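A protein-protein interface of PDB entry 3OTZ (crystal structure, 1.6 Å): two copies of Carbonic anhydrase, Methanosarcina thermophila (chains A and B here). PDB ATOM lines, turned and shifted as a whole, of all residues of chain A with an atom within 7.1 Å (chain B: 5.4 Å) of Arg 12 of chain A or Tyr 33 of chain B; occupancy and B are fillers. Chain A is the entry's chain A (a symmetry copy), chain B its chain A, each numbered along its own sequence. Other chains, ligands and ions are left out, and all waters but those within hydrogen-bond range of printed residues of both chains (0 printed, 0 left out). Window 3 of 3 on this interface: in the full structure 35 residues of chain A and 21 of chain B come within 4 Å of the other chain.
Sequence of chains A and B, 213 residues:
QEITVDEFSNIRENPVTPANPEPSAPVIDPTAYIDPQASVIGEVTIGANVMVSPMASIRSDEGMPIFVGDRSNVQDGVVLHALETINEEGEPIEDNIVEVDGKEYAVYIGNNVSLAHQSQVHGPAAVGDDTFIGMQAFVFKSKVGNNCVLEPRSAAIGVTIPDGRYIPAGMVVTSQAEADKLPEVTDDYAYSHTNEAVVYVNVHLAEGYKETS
Of the 15 printed residues of chain A, 4 touch a printed residue of chain B. Printed residues of chain A that touch a printed residue of chain B: Asn 10, Arg 12, Ser 39 and Ile 41. Along chain A the printed residues that touch a printed residue of chain B span positions 10 to 41. Along chain B the printed residues that touch a printed residue of chain A span positions 33 to 209. Among the printed residues, Asp or Glu carboxylates within 4 Å of a Lys or Arg side-chain nitrogen of the other chain: Arg 12 of chain A with Asp 35 of chain B.
OD1 of Asp 35 of chain B is in salt-bridge range of NH2 of Arg 12 of chain A (2.9 Å). The side-chain hydroxyl (OH) of Tyr 33 of chain B sits at hydrogen-bond distance from the guanidinium group (NH1) of Arg 12 of chain A (3.4 Å).
Printed residues of chain B within 4 Å of Asn 10 of chain A: Gln 37. Arg 12 of chain A touches just these residues of chain B: Tyr 33 (3.4 Å), Asp 35 (2.9 Å) and Gln 37 (3.8 Å). Of chain A, only Arg 12 (3.4 Å) comes within 4 Å of Tyr 33 of chain B. Printed residues of chain A within 4 Å of Gln 37 of chain B: Asn 10 (3.8 Å), Arg 12 (3.8 Å) and Ser 39 (3.4 Å). The nearest residue of chain A that does not touch Tyr 33 of chain B is Ile 41 of chain A (6.5 Å). The nearest printed residue of chain B that does not touch Asn 10 of chain A is Asp 35 of chain B (7.7 Å).
Among the printed residues, pairs that only touch across the chains: Ser 39 of chain A with Gln 37 of chain B (3.4 Å), Ile 41 of chain A with Tyr 209 of chain B (3.5 Å), Ser 39 of chain A with Pro 54 of chain B (3.8 Å), Asn 10 of chain A with Gln 37 of chain B (3.8 Å) and Arg 12 of chain A with Gln 37 of chain B (3.8 Å).
The backbone NH of Gly 42 of chain A sits at hydrogen-bond distance from the backbone carbonyl oxygen of Arg 12 of chain A (2.9 Å). The backbone NH (N) of Arg 12 of chain A sits at hydrogen-bond distance from the backbone carbonyl oxygen (O) of Val 40 of chain A. N of Val 40 of chain A is in hydrogen-bond range of O of Asn 10 of chain A, at 3.0 Å. The side-chain hydroxyl of Tyr 33 of chain B sits at hydrogen-bond distance from the side-chain carboxylate of Asp 35 of chain B (3.2 Å). The backbone carbonyl oxygen of Tyr 209 of chain B is in hydrogen-bond range of the side-chain hydroxyl of Thr 212 of chain B, 2.9 Å away. O of Val 52 of chain B lies within hydrogen-bond range of N of Asp 35 of chain B, at 3.0 Å.
No position is printed for both chains.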
ATOM      1  N   SER A   9      17.774   0.148 -15.615  1.00  0.00           N
ATOM      2  CA  SER A   9      17.438  -1.089 -14.914  1.00  0.00           C
ATOM      3  C   SER A   9      18.668  -1.683 -14.225  1.00  0.00           C
ATOM      4  O   SER A   9      19.803  -1.500 -14.675  1.00  0.00           O
ATOM      5  CB  SER A   9      16.828  -2.116 -15.883  1.00  0.00           C
ATOM      6  OG  SER A   9      17.729  -2.444 -16.934  1.00  0.00           O
ATOM      7  N   ASN A  10      18.425  -2.400 -13.133  1.00  0.00           N
ATOM      8  CA  ASN A  10      19.496  -3.069 -12.383  1.00  0.00           C
ATOM      9  C   ASN A  10      19.856  -4.456 -12.926  1.00  0.00           C
ATOM     10  O   ASN A  10      20.738  -5.134 -12.381  1.00  0.00           O
ATOM     11  CB  ASN A  10      19.068  -3.254 -10.935  1.00  0.00           C
ATOM     12  CG  ASN A  10      17.903  -4.221 -10.812  1.00  0.00           C
ATOM     13  OD1 ASN A  10      16.925  -4.135 -11.578  1.00  0.00           O
ATOM     14  ND2 ASN A  10      18.007  -5.165  -9.882  1.00  0.00           N
ATOM     15  N   ILE A  11      19.130  -4.917 -13.942  1.00  0.00           N
ATOM     16  CA  ILE A  11      19.533  -6.104 -14.705  1.00  0.00           C
ATOM     17  C   ILE A  11      19.899  -5.568 -16.092  1.00  0.00           C
ATOM     18  O   ILE A  11      19.062  -4.947 -16.767  1.00  0.00           O
ATOM     19  CB  ILE A  11      18.399  -7.142 -14.767  1.00  0.00           C
ATOM     20  CG1 ILE A  11      18.095  -7.654 -13.341  1.00  0.00           C
ATOM     21  CG2 ILE A  11      18.775  -8.300 -15.722  1.00  0.00           C
ATOM     22  CD1 ILE A  11      16.751  -8.367 -13.200  1.00  0.00           C
ATOM     23  N   ARG A  12      21.147  -5.784 -16.517  1.00  0.00           N
ATOM     24  CA  ARG A  12      21.698  -5.054 -17.669  1.00  0.00           C
ATOM     25  C   ARG A  12      22.607  -5.944 -18.512  1.00  0.00           C
ATOM     26  O   ARG A  12      23.182  -6.902 -18.012  1.00  0.00           O
ATOM     27  CB  ARG A  12      22.608  -3.909 -17.185  1.00  0.00           C
ATOM     28  CG  ARG A  12      21.918  -2.700 -16.631  1.00  0.00           C
ATOM     29  CD  ARG A  12      22.953  -1.608 -16.361  1.00  0.00           C
ATOM     30  NE  ARG A  12      23.341  -1.581 -14.957  1.00  0.00           N
ATOM     31  CZ  ARG A  12      24.454  -1.020 -14.484  1.00  0.00           C
ATOM     32  NH1 ARG A  12      25.324  -0.447 -15.310  1.00  0.00           N
ATOM     33  NH2 ARG A  12      24.695  -1.063 -13.178  1.00  0.00           N
ATOM     34  N   GLU A  13      22.773  -5.580 -19.772  1.00  0.00           N
ATOM     35  CA  GLU A  13      23.749  -6.227 -20.629  1.00  0.00           C
ATOM     36  C   GLU A  13      25.147  -5.723 -20.308  1.00  0.00           C
ATOM     37  O   GLU A  13      25.334  -4.625 -19.765  1.00  0.00           O
ATOM     38  CB  GLU A  13      23.419  -5.963 -22.094  1.00  0.00           C
ATOM     39  CG  GLU A  13      22.123  -6.621 -22.473  1.00  0.00           C
ATOM     40  CD  GLU A  13      21.676  -6.265 -23.858  1.00  0.00           C
ATOM     41  OE1 GLU A  13      22.384  -5.478 -24.532  1.00  0.00           O
ATOM     42  OE2 GLU A  13      20.609  -6.777 -24.266  1.00  0.00           O
ATOM     43  N   ASN A  14      26.146  -6.535 -20.633  1.00  0.00           N
ATOM     44  CA  ASN A  14      27.516  -6.061 -20.528  1.00  0.00           C
ATOM     45  C   ASN A  14      27.847  -5.232 -21.768  1.00  0.00           C
ATOM     46  O   ASN A  14      27.129  -5.261 -22.768  1.00  0.00           O
ATOM     47  CB  ASN A  14      28.510  -7.222 -20.335  1.00  0.00           C
ATOM     48  CG  ASN A  14      28.322  -8.354 -21.344  1.00  0.00           C
ATOM     49  OD1 ASN A  14      27.714  -8.177 -22.382  1.00  0.00           O
ATOM     50  ND2 ASN A  14      28.880  -9.520 -21.032  1.00  0.00           N
ATOM     51  N   SER A  24      25.746  -9.584 -23.883  1.00  0.00           N
ATOM     52  CA  SER A  24      24.861 -10.635 -23.389  1.00  0.00           C
ATOM     53  C   SER A  24      24.010 -10.051 -22.291  1.00  0.00           C
ATOM     54  O   SER A  24      24.448  -9.159 -21.568  1.00  0.00           O
ATOM     55  CB  SER A  24      25.645 -11.807 -22.792  1.00  0.00           C
ATOM     56  OG  SER A  24      26.355 -12.525 -23.778  1.00  0.00           O
ATOM     57  N   ALA A  25      22.788 -10.548 -22.184  1.00  0.00           N
ATOM     58  CA  ALA A  25      21.905 -10.164 -21.106  1.00  0.00           C
ATOM     59  C   ALA A  25      21.721 -11.382 -20.191  1.00  0.00           C
ATOM     60  O   ALA A  25      21.800 -12.534 -20.641  1.00  0.00           O
ATOM     61  CB  ALA A  25      20.560  -9.689 -21.661  1.00  0.00           C
ATOM     62  N   PRO A  26      21.491 -11.120 -18.903  1.00  0.00           N
ATOM     63  CA  PRO A  26      21.330 -12.220 -17.948  1.00  0.00           C
ATOM     64  C   PRO A  26      20.159 -13.122 -18.305  1.00  0.00           C
ATOM     65  O   PRO A  26      19.153 -12.618 -18.832  1.00  0.00           O
ATOM     66  CB  PRO A  26      21.030 -11.484 -16.647  1.00  0.00           C
ATOM     67  CG  PRO A  26      21.774 -10.155 -16.788  1.00  0.00           C
ATOM     68  CD  PRO A  26      21.561  -9.801 -18.236  1.00  0.00           C
ATOM     69  N   SER A  39      22.568  -5.695  -8.281  1.00  0.00           N
ATOM     70  CA  SER A  39      22.997  -5.416  -9.660  1.00  0.00           C
ATOM     71  C   SER A  39      23.403  -6.746 -10.324  1.00  0.00           C
ATOM     72  O   SER A  39      24.194  -7.486  -9.764  1.00  0.00           O
ATOM     73  CB  SER A  39      24.206  -4.475  -9.649  1.00  0.00           C
ATOM     74  OG  SER A  39      24.661  -4.240 -10.977  1.00  0.00           O
ATOM     75  N   VAL A  40      22.841  -7.031 -11.506  1.00  0.00           N
ATOM     76  CA  VAL A  40      23.204  -8.222 -12.259  1.00  0.00           C
ATOM     77  C   VAL A  40      23.496  -7.760 -13.684  1.00  0.00           C
ATOM     78  O   VAL A  40      22.594  -7.255 -14.386  1.00  0.00           O
ATOM     79  CB  VAL A  40      22.049  -9.252 -12.299  1.00  0.00           C
ATOM     80  CG1 VAL A  40      22.519 -10.507 -12.984  1.00  0.00           C
ATOM     81  CG2 VAL A  40      21.610  -9.598 -10.862  1.00  0.00           C
ATOM     82  N   ILE A  41      24.737  -7.975 -14.135  1.00  0.00           N
ATOM     83  CA  ILE A  41      25.185  -7.438 -15.429  1.00  0.00           C
ATOM     84  C   ILE A  41      25.822  -8.540 -16.247  1.00  0.00           C
ATOM     85  O   ILE A  41      26.693  -9.247 -15.736  1.00  0.00           O
ATOM     86  CB  ILE A  41      26.277  -6.350 -15.183  1.00  0.00           C
ATOM     87  CG1 ILE A  41      25.645  -5.128 -14.527  1.00  0.00           C
ATOM     88  CG2 ILE A  41      26.940  -5.937 -16.515  1.00  0.00           C
ATOM     89  CD1 ILE A  41      26.695  -4.063 -14.105  1.00  0.00           C
ATOM     90  N   GLY A  42      25.389  -8.704 -17.491  1.00  0.00           N
ATOM     91  CA  GLY A  42      26.164  -9.457 -18.464  1.00  0.00           C
ATOM     92  C   GLY A  42      25.827 -10.928 -18.553  1.00  0.00           C
ATOM     93  O   GLY A  42      24.677 -11.342 -18.419  1.00  0.00           O
ATOM     94  N   GLU A  43      26.844 -11.733 -18.826  1.00  0.00           N
ATOM     95  CA  GLU A  43      26.595 -13.118 -19.214  1.00  0.00           C
ATOM     96  C   GLU A  43      26.485 -13.934 -17.923  1.00  0.00           C
ATOM     97  O   GLU A  43      27.465 -14.490 -17.421  1.00  0.00           O
ATOM     98  CB  GLU A  43      27.729 -13.623 -20.109  1.00  0.00           C
ATOM     99  CG  GLU A  43      27.396 -14.953 -20.766  1.00  0.00           C
ATOM    100  CD  GLU A  43      28.543 -15.490 -21.618  1.00  0.00           C
ATOM    101  OE1 GLU A  43      29.546 -14.770 -21.806  1.00  0.00           O
ATOM    102  OE2 GLU A  43      28.416 -16.631 -22.098  1.00  0.00           O
ATOM    103  N   VAL A  44      25.279 -13.949 -17.361  1.00  0.00           N
ATOM    104  CA  VAL A  44      25.001 -14.577 -16.075  1.00  0.00           C
ATOM    105  C   VAL A  44      23.770 -15.471 -16.274  1.00  0.00           C
ATOM    106  O   VAL A  44      22.823 -15.063 -16.933  1.00  0.00           O
ATOM    107  CB  VAL A  44      24.605 -13.490 -15.050  1.00  0.00           C
ATOM    108  CG1 VAL A  44      24.144 -14.135 -13.728  1.00  0.00           C
ATOM    109  CG2 VAL A  44      25.778 -12.491 -14.833  1.00  0.00           C
ATOM    110  N   THR B  31      35.580  11.582 -19.126  1.00  0.00           N
ATOM    111  CA  THR B  31      35.854  10.228 -19.624  1.00  0.00           C
ATOM    112  C   THR B  31      35.717   9.170 -18.540  1.00  0.00           C
ATOM    113  O   THR B  31      35.889   7.985 -18.800  1.00  0.00           O
ATOM    114  CB  THR B  31      37.262  10.059 -20.214  1.00  0.00           C
ATOM    115  OG1 THR B  31      38.248  10.288 -19.211  1.00  0.00           O
ATOM    116  CG2 THR B  31      37.508  11.025 -21.401  1.00  0.00           C
ATOM    117  N   ALA B  32      35.407   9.580 -17.319  1.00  0.00           N
ATOM    118  CA  ALA B  32      35.188   8.592 -16.272  1.00  0.00           C
ATOM    119  C   ALA B  32      33.785   7.997 -16.388  1.00  0.00           C
ATOM    120  O   ALA B  32      32.847   8.650 -16.858  1.00  0.00           O
ATOM    121  CB  ALA B  32      35.369   9.233 -14.913  1.00  0.00           C
ATOM    122  N   TYR B  33      33.625   6.749 -15.939  1.00  0.00           N
ATOM    123  CA  TYR B  33      32.291   6.124 -15.898  1.00  0.00           C
ATOM    124  C   TYR B  33      31.934   5.888 -14.415  1.00  0.00           C
ATOM    125  O   TYR B  33      32.660   5.182 -13.705  1.00  0.00           O
ATOM    126  CB  TYR B  33      32.300   4.769 -16.621  1.00  0.00           C
ATOM    127  CG  TYR B  33      30.982   4.073 -16.453  1.00  0.00           C
ATOM    128  CD1 TYR B  33      29.864   4.537 -17.119  1.00  0.00           C
ATOM    129  CD2 TYR B  33      30.855   2.973 -15.611  1.00  0.00           C
ATOM    130  CE1 TYR B  33      28.620   3.912 -16.951  1.00  0.00           C
ATOM    131  CE2 TYR B  33      29.623   2.350 -15.426  1.00  0.00           C
ATOM    132  CZ  TYR B  33      28.529   2.815 -16.085  1.00  0.00           C
ATOM    133  OH  TYR B  33      27.305   2.196 -15.918  1.00  0.00           O
ATOM    134  N   ILE B  34      30.816   6.456 -13.983  1.00  0.00           N
ATOM    135  CA  ILE B  34      30.303   6.233 -12.630  1.00  0.00           C
ATOM    136  C   ILE B  34      29.018   5.403 -12.758  1.00  0.00           C
ATOM    137  O   ILE B  34      28.011   5.858 -13.343  1.00  0.00           O
ATOM    138  CB  ILE B  34      29.935   7.562 -11.967  1.00  0.00           C
ATOM    139  CG1 ILE B  34      31.105   8.582 -12.057  1.00  0.00           C
ATOM    140  CG2 ILE B  34      29.486   7.320 -10.483  1.00  0.00           C
ATOM    141  CD1 ILE B  34      32.373   8.142 -11.438  1.00  0.00           C
ATOM    142  N   ASP B  35      29.021   4.181 -12.229  1.00  0.00           N
ATOM    143  CA  ASP B  35      27.845   3.342 -12.364  1.00  0.00           C
ATOM    144  C   ASP B  35      26.677   3.994 -11.639  1.00  0.00           C
ATOM    145  O   ASP B  35      26.849   4.607 -10.594  1.00  0.00           O
ATOM    146  CB  ASP B  35      28.136   1.963 -11.750  1.00  0.00           C
ATOM    147  CG  ASP B  35      27.085   0.964 -12.125  1.00  0.00           C
ATOM    148  OD1 ASP B  35      27.213   0.404 -13.224  1.00  0.00           O
ATOM    149  OD2 ASP B  35      26.110   0.789 -11.371  1.00  0.00           O
ATOM    150  N   PRO B  36      25.478   3.875 -12.185  1.00  0.00           N
ATOM    151  CA  PRO B  36      24.304   4.455 -11.518  1.00  0.00           C
ATOM    152  C   PRO B  36      24.055   3.877 -10.131  1.00  0.00           C
ATOM    153  O   PRO B  36      23.381   4.526  -9.334  1.00  0.00           O
ATOM    154  CB  PRO B  36      23.144   4.050 -12.437  1.00  0.00           C
ATOM    155  CG  PRO B  36      23.763   3.848 -13.767  1.00  0.00           C
ATOM    156  CD  PRO B  36      25.174   3.336 -13.529  1.00  0.00           C
ATOM    157  N   GLN B  37      24.570   2.672  -9.852  1.00  0.00           N
ATOM    158  CA  GLN B  37      24.395   2.083  -8.534  1.00  0.00           C
ATOM    159  C   GLN B  37      25.603   2.280  -7.628  1.00  0.00           C
ATOM    160  O   GLN B  37      25.684   1.658  -6.560  1.00  0.00           O
ATOM    161  CB  GLN B  37      24.027   0.591  -8.651  1.00  0.00           C
ATOM    162  CG  GLN B  37      22.559   0.453  -9.092  1.00  0.00           C
ATOM    163  CD  GLN B  37      22.094  -0.996  -9.253  1.00  0.00           C
ATOM    164  OE1 GLN B  37      22.392  -1.622 -10.243  1.00  0.00           O
ATOM    165  NE2 GLN B  37      21.311  -1.485  -8.306  1.00  0.00           N
ATOM    166  N   VAL B  50      38.541   6.697 -15.341  1.00  0.00           N
ATOM    167  CA  VAL B  50      38.306   5.913 -14.119  1.00  0.00           C
ATOM    168  C   VAL B  50      36.985   5.169 -14.232  1.00  0.00           C
ATOM    169  O   VAL B  50      36.019   5.713 -14.726  1.00  0.00           O
ATOM    170  CB  VAL B  50      38.283   6.872 -12.919  1.00  0.00           C
ATOM    171  CG1 VAL B  50      37.718   6.164 -11.656  1.00  0.00           C
ATOM    172  CG2 VAL B  50      39.697   7.422 -12.658  1.00  0.00           C
ATOM    173  N   MET B  51      36.959   3.921 -13.765  1.00  0.00           N
ATOM    174  CA  MET B  51      35.737   3.135 -13.696  1.00  0.00           C
ATOM    175  C   MET B  51      35.290   2.951 -12.252  1.00  0.00           C
ATOM    176  O   MET B  51      36.041   2.360 -11.483  1.00  0.00           O
ATOM    177  CB  MET B  51      36.010   1.748 -14.247  1.00  0.00           C
ATOM    178  CG  MET B  51      34.900   0.778 -13.901  1.00  0.00           C
ATOM    179  SD  MET B  51      33.798   0.695 -15.285  1.00  0.00           S
ATOM    180  CE  MET B  51      34.038  -1.002 -15.716  1.00  0.00           C
ATOM    181  N   VAL B  52      34.091   3.427 -11.900  1.00  0.00           N
ATOM    182  CA  VAL B  52      33.536   3.250 -10.563  1.00  0.00           C
ATOM    183  C   VAL B  52      32.348   2.296 -10.695  1.00  0.00           C
ATOM    184  O   VAL B  52      31.365   2.595 -11.394  1.00  0.00           O
ATOM    185  CB  VAL B  52      33.114   4.578  -9.928  1.00  0.00           C
ATOM    186  CG1 VAL B  52      32.512   4.347  -8.512  1.00  0.00           C
ATOM    187  CG2 VAL B  52      34.314   5.530  -9.825  1.00  0.00           C
ATOM    188  N   PRO B  54      29.359  -0.809  -9.551  1.00  0.00           N
ATOM    189  CA  PRO B  54      28.180  -0.864  -8.682  1.00  0.00           C
ATOM    190  C   PRO B  54      28.548  -1.068  -7.224  1.00  0.00           C
ATOM    191  O   PRO B  54      29.461  -1.823  -6.870  1.00  0.00           O
ATOM    192  CB  PRO B  54      27.421  -2.100  -9.198  1.00  0.00           C
ATOM    193  CG  PRO B  54      27.851  -2.269 -10.656  1.00  0.00           C
ATOM    194  CD  PRO B  54      29.284  -1.768 -10.688  1.00  0.00           C
ATOM    195  N   ALA B 206      35.503   0.978 -18.914  1.00  0.00           N
ATOM    196  CA  ALA B 206      34.943   2.310 -18.694  1.00  0.00           C
ATOM    197  C   ALA B 206      34.436   2.872 -20.017  1.00  0.00           C
ATOM    198  O   ALA B 206      33.349   3.447 -20.077  1.00  0.00           O
ATOM    199  CB  ALA B 206      35.988   3.237 -18.062  1.00  0.00           C
ATOM    200  N   TYR B 209      31.236   0.958 -21.071  1.00  0.00           N
ATOM    201  CA  TYR B 209      30.052   1.319 -20.283  1.00  0.00           C
ATOM    202  C   TYR B 209      29.600   2.728 -20.639  1.00  0.00           C
ATOM    203  O   TYR B 209      28.410   3.002 -20.653  1.00  0.00           O
ATOM    204  CB  TYR B 209      30.289   1.226 -18.775  1.00  0.00           C
ATOM    205  CG  TYR B 209      30.192  -0.193 -18.222  1.00  0.00           C
ATOM    206  CD1 TYR B 209      31.324  -0.874 -17.790  1.00  0.00           C
ATOM    207  CD2 TYR B 209      28.969  -0.835 -18.158  1.00  0.00           C
ATOM    208  CE1 TYR B 209      31.234  -2.195 -17.274  1.00  0.00           C
ATOM    209  CE2 TYR B 209      28.863  -2.128 -17.663  1.00  0.00           C
ATOM    210  CZ  TYR B 209      29.991  -2.789 -17.224  1.00  0.00           C
ATOM    211  OH  TYR B 209      29.862  -4.088 -16.753  1.00  0.00           O
ATOM    212  N   LYS B 210      30.538   3.620 -20.936  1.00  0.00           N
ATOM    213  CA  LYS B 210      30.134   4.966 -21.350  1.00  0.00           C
ATOM    214  C   LYS B 210      29.298   4.958 -22.619  1.00  0.00           C
ATOM    215  O   LYS B 210      28.470   5.832 -22.815  1.00  0.00           O
ATOM    216  CB  LYS B 210      31.376   5.835 -21.577  1.00  0.00           C
ATOM    217  CG  LYS B 210      32.021   6.255 -20.281  1.00  0.00           C
ATOM    218  CD  LYS B 210      31.155   7.286 -19.579  1.00  0.00           C
ATOM    219  CE  LYS B 210      31.551   8.688 -19.957  1.00  0.00           C
ATOM    220  NZ  LYS B 210      30.994   9.628 -18.963  1.00  0.00           N
ATOM    221  N   THR B 212      27.048   2.931 -23.401  1.00  0.00           N
ATOM    222  CA  THR B 212      25.713   2.382 -23.098  1.00  0.00           C
ATOM    223  C   THR B 212      24.882   3.367 -22.295  1.00  0.00           C
ATOM    224  O   THR B 212      23.735   3.079 -21.976  1.00  0.00           O
ATOM    225  CB  THR B 212      25.773   1.086 -22.221  1.00  0.00           C
ATOM    226  OG1 THR B 212      25.964   1.436 -20.834  1.00  0.00           O
ATOM    227  CG2 THR B 212      26.891   0.156 -22.654  1.00  0.00           C
ATOM    228  N   SER B 213      25.456   4.538 -22.012  1.00  0.00           N
ATOM    229  CA  SER B 213      24.824   5.536 -21.152  1.00  0.00           C
ATOM    230  C   SER B 213      24.194   6.670 -21.951  1.00  0.00           C
ATOM    231  O   SER B 213      23.206   7.287 -21.546  1.00  0.00           O
ATOM    232  CB  SER B 213      25.877   6.120 -20.210  1.00  0.00           C
ATOM    233  OG  SER B 213      26.579   5.086 -19.547  1.00  0.00           O
ATOM    234  OXT SER B 213      24.667   7.018 -23.019  1.00  0.00           O
